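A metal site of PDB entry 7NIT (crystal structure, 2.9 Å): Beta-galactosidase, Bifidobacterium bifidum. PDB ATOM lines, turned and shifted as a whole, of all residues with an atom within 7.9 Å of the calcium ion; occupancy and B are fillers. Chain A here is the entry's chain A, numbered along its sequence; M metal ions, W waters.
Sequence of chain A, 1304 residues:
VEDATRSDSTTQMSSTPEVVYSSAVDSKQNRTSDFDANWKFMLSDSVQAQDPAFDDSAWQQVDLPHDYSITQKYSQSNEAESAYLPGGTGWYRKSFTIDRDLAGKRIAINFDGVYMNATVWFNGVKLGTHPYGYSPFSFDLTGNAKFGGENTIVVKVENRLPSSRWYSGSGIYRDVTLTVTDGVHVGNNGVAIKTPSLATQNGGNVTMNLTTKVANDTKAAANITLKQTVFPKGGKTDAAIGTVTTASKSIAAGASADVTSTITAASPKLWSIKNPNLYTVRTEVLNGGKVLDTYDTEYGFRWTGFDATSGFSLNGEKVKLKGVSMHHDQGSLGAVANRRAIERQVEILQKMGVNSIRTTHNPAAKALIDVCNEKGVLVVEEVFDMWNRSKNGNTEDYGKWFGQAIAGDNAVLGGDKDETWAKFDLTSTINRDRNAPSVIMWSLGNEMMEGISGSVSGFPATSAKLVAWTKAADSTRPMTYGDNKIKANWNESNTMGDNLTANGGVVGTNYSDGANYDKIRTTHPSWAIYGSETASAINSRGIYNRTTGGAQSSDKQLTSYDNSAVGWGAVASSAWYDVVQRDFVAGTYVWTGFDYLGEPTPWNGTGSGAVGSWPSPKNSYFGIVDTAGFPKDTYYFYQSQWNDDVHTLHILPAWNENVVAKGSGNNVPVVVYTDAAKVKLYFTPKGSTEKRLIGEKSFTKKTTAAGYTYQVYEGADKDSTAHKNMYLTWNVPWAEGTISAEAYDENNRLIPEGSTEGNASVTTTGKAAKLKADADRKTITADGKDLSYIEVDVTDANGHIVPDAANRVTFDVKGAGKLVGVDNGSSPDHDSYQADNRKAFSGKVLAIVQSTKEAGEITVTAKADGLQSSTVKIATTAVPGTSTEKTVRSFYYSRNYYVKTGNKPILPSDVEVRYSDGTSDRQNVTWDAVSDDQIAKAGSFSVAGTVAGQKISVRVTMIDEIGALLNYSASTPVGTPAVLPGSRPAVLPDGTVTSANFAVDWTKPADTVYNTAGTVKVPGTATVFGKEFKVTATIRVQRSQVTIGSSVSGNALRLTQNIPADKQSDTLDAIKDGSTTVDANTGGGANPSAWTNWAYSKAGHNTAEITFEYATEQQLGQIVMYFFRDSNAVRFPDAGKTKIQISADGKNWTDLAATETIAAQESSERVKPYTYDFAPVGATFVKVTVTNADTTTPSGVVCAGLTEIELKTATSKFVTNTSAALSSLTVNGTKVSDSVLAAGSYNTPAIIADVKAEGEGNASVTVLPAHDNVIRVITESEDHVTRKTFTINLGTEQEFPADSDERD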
ATOM      1  N   THR A1067     -13.806 -23.197  35.327  1.00  0.00           N
ATOM      2  CA  THR A1067     -12.731 -24.016  34.794  1.00  0.00           C
ATOM      3  C   THR A1067     -11.579 -23.151  34.303  1.00  0.00           C
ATOM      4  O   THR A1067     -11.764 -22.277  33.452  1.00  0.00           O
ATOM      5  CB  THR A1067     -13.239 -24.913  33.657  1.00  0.00           C
ATOM      6  OG1 THR A1067     -13.849 -24.054  32.685  1.00  0.00           O
ATOM      7  CG2 THR A1067     -14.247 -25.952  34.117  1.00  0.00           C
ATOM      8  N   LEU A1068     -10.372 -23.379  34.848  1.00  0.00           N
ATOM      9  CA  LEU A1068      -9.210 -22.554  34.556  1.00  0.00           C
ATOM     10  C   LEU A1068      -8.686 -22.849  33.149  1.00  0.00           C
ATOM     11  O   LEU A1068      -8.485 -21.922  32.357  1.00  0.00           O
ATOM     12  CB  LEU A1068      -8.137 -22.765  35.633  1.00  0.00           C
ATOM     13  CG  LEU A1068      -6.777 -22.089  35.398  1.00  0.00           C
ATOM     14  CD1 LEU A1068      -6.869 -20.577  35.207  1.00  0.00           C
ATOM     15  CD2 LEU A1068      -5.817 -22.432  36.515  1.00  0.00           C
ATOM     16  N   ASP A1069      -8.502 -24.151  32.844  1.00  0.00           N
ATOM     17  CA  ASP A1069      -7.885 -24.598  31.610  1.00  0.00           C
ATOM     18  C   ASP A1069      -8.625 -24.059  30.393  1.00  0.00           C
ATOM     19  O   ASP A1069      -8.146 -24.217  29.273  1.00  0.00           O
ATOM     20  CB  ASP A1069      -7.757 -26.121  31.559  1.00  0.00           C
ATOM     21  CG  ASP A1069      -6.568 -26.613  32.385  1.00  0.00           C
ATOM     22  OD1 ASP A1069      -6.092 -25.842  33.234  1.00  0.00           O
ATOM     23  OD2 ASP A1069      -6.112 -27.741  32.156  1.00  0.00           O
ATOM     24  N   ALA A1070      -9.781 -23.437  30.632  1.00  0.00           N
ATOM     25  CA  ALA A1070     -10.614 -22.890  29.572  1.00  0.00           C
ATOM     26  C   ALA A1070      -9.930 -21.716  28.902  1.00  0.00           C
ATOM     27  O   ALA A1070     -10.297 -21.372  27.784  1.00  0.00           O
ATOM     28  CB  ALA A1070     -11.950 -22.489  30.139  1.00  0.00           C
ATOM     29  N   ILE A1071      -8.933 -21.103  29.574  1.00  0.00           N
ATOM     30  CA  ILE A1071      -8.383 -19.832  29.138  1.00  0.00           C
ATOM     31  C   ILE A1071      -7.290 -20.031  28.089  1.00  0.00           C
ATOM     32  O   ILE A1071      -6.804 -19.051  27.531  1.00  0.00           O
ATOM     33  CB  ILE A1071      -7.957 -18.900  30.294  1.00  0.00           C
ATOM     34  CG1 ILE A1071      -6.690 -19.384  31.001  1.00  0.00           C
ATOM     35  CG2 ILE A1071      -9.103 -18.635  31.255  1.00  0.00           C
ATOM     36  CD1 ILE A1071      -6.306 -18.570  32.218  1.00  0.00           C
ATOM     37  N   LYS A1072      -6.934 -21.292  27.813  1.00  0.00           N
ATOM     38  CA  LYS A1072      -5.967 -21.662  26.773  1.00  0.00           C
ATOM     39  C   LYS A1072      -6.604 -22.563  25.697  1.00  0.00           C
ATOM     40  O   LYS A1072      -5.913 -23.083  24.835  1.00  0.00           O
ATOM     41  CB  LYS A1072      -4.700 -22.275  27.381  1.00  0.00           C
ATOM     42  CG  LYS A1072      -4.926 -23.167  28.581  1.00  0.00           C
ATOM     43  CD  LYS A1072      -3.818 -24.137  28.871  1.00  0.00           C
ATOM     44  CE  LYS A1072      -4.403 -25.488  29.210  1.00  0.00           C
ATOM     45  NZ  LYS A1072      -3.347 -26.362  29.782  1.00  0.00           N
ATOM     46  N   ASP A1073      -7.922 -22.692  25.714  1.00  0.00           N
ATOM     47  CA  ASP A1073      -8.635 -23.598  24.815  1.00  0.00           C
ATOM     48  C   ASP A1073      -8.806 -23.005  23.419  1.00  0.00           C
ATOM     49  O   ASP A1073      -9.378 -23.646  22.546  1.00  0.00           O
ATOM     50  CB  ASP A1073      -9.953 -24.093  25.425  1.00  0.00           C
ATOM     51  CG  ASP A1073     -11.081 -23.081  25.443  1.00  0.00           C
ATOM     52  OD1 ASP A1073     -10.960 -22.007  24.801  1.00  0.00           O
ATOM     53  OD2 ASP A1073     -12.087 -23.372  26.128  1.00  0.00           O
ATOM     54  N   GLY A1074      -8.356 -21.770  23.204  1.00  0.00           N
ATOM     55  CA  GLY A1074      -8.381 -21.167  21.881  1.00  0.00           C
ATOM     56  C   GLY A1074      -9.724 -20.545  21.488  1.00  0.00           C
ATOM     57  O   GLY A1074      -9.813 -20.019  20.387  1.00  0.00           O
ATOM     58  N   SER A1075     -10.746 -20.592  22.360  1.00  0.00           N
ATOM     59  CA  SER A1075     -12.027 -19.947  22.120  1.00  0.00           C
ATOM     60  C   SER A1075     -12.245 -18.769  23.088  1.00  0.00           C
ATOM     61  O   SER A1075     -11.790 -18.823  24.219  1.00  0.00           O
ATOM     62  CB  SER A1075     -13.139 -20.952  22.225  1.00  0.00           C
ATOM     63  OG  SER A1075     -14.435 -20.346  22.147  1.00  0.00           O
ATOM     64  N   THR A1076     -12.945 -17.719  22.610  1.00  0.00           N
ATOM     65  CA  THR A1076     -13.036 -16.463  23.360  1.00  0.00           C
ATOM     66  C   THR A1076     -14.433 -16.223  23.962  1.00  0.00           C
ATOM     67  O   THR A1076     -14.584 -15.332  24.787  1.00  0.00           O
ATOM     68  CB  THR A1076     -12.624 -15.244  22.525  1.00  0.00           C
ATOM     69  OG1 THR A1076     -13.742 -14.763  21.764  1.00  0.00           O
ATOM     70  CG2 THR A1076     -11.404 -15.445  21.659  1.00  0.00           C
ATOM     71  N   THR A1077     -15.450 -16.977  23.536  1.00  0.00           N
ATOM     72  CA  THR A1077     -16.844 -16.697  23.853  1.00  0.00           C
ATOM     73  C   THR A1077     -17.203 -17.291  25.213  1.00  0.00           C
ATOM     74  O   THR A1077     -16.528 -18.208  25.683  1.00  0.00           O
ATOM     75  CB  THR A1077     -17.752 -17.279  22.762  1.00  0.00           C
ATOM     76  OG1 THR A1077     -18.055 -18.632  23.097  1.00  0.00           O
ATOM     77  CG2 THR A1077     -17.177 -17.224  21.351  1.00  0.00           C
ATOM     78  N   VAL A1078     -18.299 -16.777  25.828  1.00  0.00           N
ATOM     79  CA  VAL A1078     -18.814 -17.329  27.084  1.00  0.00           C
ATOM     80  C   VAL A1078     -20.085 -18.120  26.832  1.00  0.00           C
ATOM     81  O   VAL A1078     -20.982 -17.618  26.148  1.00  0.00           O
ATOM     82  CB  VAL A1078     -19.146 -16.252  28.140  1.00  0.00           C
ATOM     83  CG1 VAL A1078     -18.577 -16.630  29.504  1.00  0.00           C
ATOM     84  CG2 VAL A1078     -18.725 -14.859  27.702  1.00  0.00           C
ATOM     85  N   PRO A1088     -17.926 -24.272  31.838  1.00  0.00           N
ATOM     86  CA  PRO A1088     -16.849 -24.974  31.132  1.00  0.00           C
ATOM     87  C   PRO A1088     -16.081 -24.076  30.166  1.00  0.00           C
ATOM     88  O   PRO A1088     -15.045 -24.511  29.654  1.00  0.00           O
ATOM     89  CB  PRO A1088     -17.636 -26.006  30.315  1.00  0.00           C
ATOM     90  CG  PRO A1088     -18.961 -25.319  30.008  1.00  0.00           C
ATOM     91  CD  PRO A1088     -19.255 -24.523  31.258  1.00  0.00           C
ATOM     92  N   SER A1089     -16.583 -22.861  29.907  1.00  0.00           N
ATOM     93  CA  SER A1089     -16.065 -21.996  28.853  1.00  0.00           C
ATOM     94  C   SER A1089     -15.069 -20.989  29.389  1.00  0.00           C
ATOM     95  O   SER A1089     -14.276 -20.454  28.604  1.00  0.00           O
ATOM     96  CB  SER A1089     -17.164 -21.297  28.086  1.00  0.00           C
ATOM     97  OG  SER A1089     -17.711 -20.207  28.834  1.00  0.00           O
ATOM     98  N   ALA A1090     -15.107 -20.730  30.700  1.00  0.00           N
ATOM     99  CA  ALA A1090     -14.411 -19.573  31.265  1.00  0.00           C
ATOM    100  C   ALA A1090     -13.947 -19.864  32.686  1.00  0.00           C
ATOM    101  O   ALA A1090     -14.354 -20.852  33.303  1.00  0.00           O
ATOM    102  CB  ALA A1090     -15.337 -18.357  31.216  1.00  0.00           C
ATOM    103  N   TRP A1091     -13.074 -18.961  33.170  1.00  0.00           N
ATOM    104  CA  TRP A1091     -12.617 -18.912  34.555  1.00  0.00           C
ATOM    105  C   TRP A1091     -13.155 -17.658  35.228  1.00  0.00           C
ATOM    106  O   TRP A1091     -13.428 -16.656  34.563  1.00  0.00           O
ATOM    107  CB  TRP A1091     -11.086 -18.938  34.580  1.00  0.00           C
ATOM    108  CG  TRP A1091     -10.463 -18.578  35.898  1.00  0.00           C
ATOM    109  CD1 TRP A1091      -9.958 -19.442  36.822  1.00  0.00           C
ATOM    110  CD2 TRP A1091     -10.231 -17.255  36.421  1.00  0.00           C
ATOM    111  NE1 TRP A1091      -9.439 -18.758  37.885  1.00  0.00           N
ATOM    112  CE2 TRP A1091      -9.591 -17.422  37.673  1.00  0.00           C
ATOM    113  CE3 TRP A1091     -10.483 -15.963  35.957  1.00  0.00           C
ATOM    114  CZ2 TRP A1091      -9.231 -16.329  38.464  1.00  0.00           C
ATOM    115  CZ3 TRP A1091     -10.126 -14.888  36.739  1.00  0.00           C
ATOM    116  CH2 TRP A1091      -9.503 -15.079  37.975  1.00  0.00           C
ATOM    117  N   TYR A1122      -9.337 -11.758  27.267  1.00  0.00           N
ATOM    118  CA  TYR A1122     -10.760 -11.728  26.950  1.00  0.00           C
ATOM    119  C   TYR A1122     -11.525 -11.841  28.263  1.00  0.00           C
ATOM    120  O   TYR A1122     -11.884 -12.941  28.694  1.00  0.00           O
ATOM    121  CB  TYR A1122     -11.115 -12.833  25.928  1.00  0.00           C
ATOM    122  CG  TYR A1122     -10.648 -12.532  24.533  1.00  0.00           C
ATOM    123  CD1 TYR A1122      -9.337 -12.784  24.143  1.00  0.00           C
ATOM    124  CD2 TYR A1122     -11.493 -11.947  23.595  1.00  0.00           C
ATOM    125  CE1 TYR A1122      -8.888 -12.478  22.869  1.00  0.00           C
ATOM    126  CE2 TYR A1122     -11.058 -11.646  22.316  1.00  0.00           C
ATOM    127  CZ  TYR A1122      -9.765 -11.908  21.949  1.00  0.00           C
ATOM    128  OH  TYR A1122      -9.348 -11.573  20.692  1.00  0.00           O
ATOM    129  N   LEU A1202     -12.557 -14.451  32.846  1.00  0.00           N
ATOM    130  CA  LEU A1202     -11.779 -14.614  31.619  1.00  0.00           C
ATOM    131  C   LEU A1202     -12.250 -15.860  30.865  1.00  0.00           C
ATOM    132  O   LEU A1202     -12.403 -16.929  31.463  1.00  0.00           O
ATOM    133  CB  LEU A1202     -10.322 -14.809  32.018  1.00  0.00           C
ATOM    134  CG  LEU A1202      -9.563 -13.550  32.422  1.00  0.00           C
ATOM    135  CD1 LEU A1202      -8.296 -13.963  33.189  1.00  0.00           C
ATOM    136  CD2 LEU A1202      -9.238 -12.680  31.197  1.00  0.00           C
ATOM    137  N   THR A1203     -12.426 -15.718  29.542  1.00  0.00           N
ATOM    138  CA  THR A1203     -12.608 -16.842  28.639  1.00  0.00           C
ATOM    139  C   THR A1203     -11.273 -17.299  28.051  1.00  0.00           C
ATOM    140  O   THR A1203     -11.070 -18.482  27.795  1.00  0.00           O
ATOM    141  CB  THR A1203     -13.557 -16.511  27.478  1.00  0.00           C
ATOM    142  OG1 THR A1203     -12.904 -15.538  26.658  1.00  0.00           O
ATOM    143  CG2 THR A1203     -14.918 -16.023  27.932  1.00  0.00           C
ATOM    144  N   GLU A1204     -10.354 -16.351  27.825  1.00  0.00           N
ATOM    145  CA  GLU A1204      -9.081 -16.628  27.172  1.00  0.00           C
ATOM    146  C   GLU A1204      -8.036 -15.580  27.577  1.00  0.00           C
ATOM    147  O   GLU A1204      -8.350 -14.411  27.757  1.00  0.00           O
ATOM    148  CB  GLU A1204      -9.266 -16.596  25.654  1.00  0.00           C
ATOM    149  CG  GLU A1204      -8.152 -17.289  24.878  1.00  0.00           C
ATOM    150  CD  GLU A1204      -8.123 -18.811  24.955  1.00  0.00           C
ATOM    151  OE1 GLU A1204      -9.075 -19.421  25.518  1.00  0.00           O
ATOM    152  OE2 GLU A1204      -7.115 -19.389  24.461  1.00  0.00           O
ATOM    153  N   ILE A1205      -6.781 -16.033  27.701  1.00  0.00           N
ATOM    154  CA  ILE A1205      -5.599 -15.185  27.699  1.00  0.00           C
ATOM    155  C   ILE A1205      -4.696 -15.676  26.560  1.00  0.00           C
ATOM    156  O   ILE A1205      -4.075 -16.714  26.675  1.00  0.00           O
ATOM    157  CB  ILE A1205      -4.880 -15.261  29.061  1.00  0.00           C
ATOM    158  CG1 ILE A1205      -5.669 -14.590  30.177  1.00  0.00           C
ATOM    159  CG2 ILE A1205      -3.463 -14.708  28.975  1.00  0.00           C
ATOM    160  CD1 ILE A1205      -5.066 -14.818  31.551  1.00  0.00           C
HETATM  161 CA    CA M   1     -11.233 -20.098  26.102  1.00  0.00          CA
HETATM  162  O   HOH W   1     -13.520 -20.671  26.103  1.00  0.00           O
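The side-chain carboxylate of Glu 1204 sits at hydrogen-bond distance from the backbone NH of Gly 1074, at 3.0 Å. O of Glu 1204 is in hydrogen-bond range of N of Tyr 1122, 2.9 Å away. OG1 of Thr 1203 lies within hydrogen-bond range of O of Thr 1076, at 2.5 Å. O of Tyr 1122 sits at hydrogen-bond distance from N of Thr 1203 (3.0 Å).
The calcium ion is bound by the backbone carbonyl oxygen (O) of Ala 1070 (2.3 Å), the side-chain carboxylate (OD1) of Asp 1073 (2.3 Å), the side-chain carboxylate (OE1) of Glu 1204 (2.3 Å), the backbone carbonyl oxygen (O) of Ser 1075 (2.3 Å), the backbone carbonyl oxygen (O) of Thr 1203 (2.3 Å) and water W1 (2.4 Å). The calcium ion has six donor atoms within binding distance.
Water W1 lies within hydrogen-bond range of the backbone carbonyl oxygen (O) of Ser 1089 (2.6 Å) and the side-chain carboxylate (OD2) of Asp 1073 (3.1 Å).
Ser 1089 touches the calcium ion (O to CA, 3.96 Å). Within 4 Å of the calcium ion: Ala 1070, Asp 1073, Ser 1075, Ser 1089, Thr 1203 and Glu 1204. The nearest printed residue that does not touch the calcium ion is Ile 1071 (4.2 Å).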
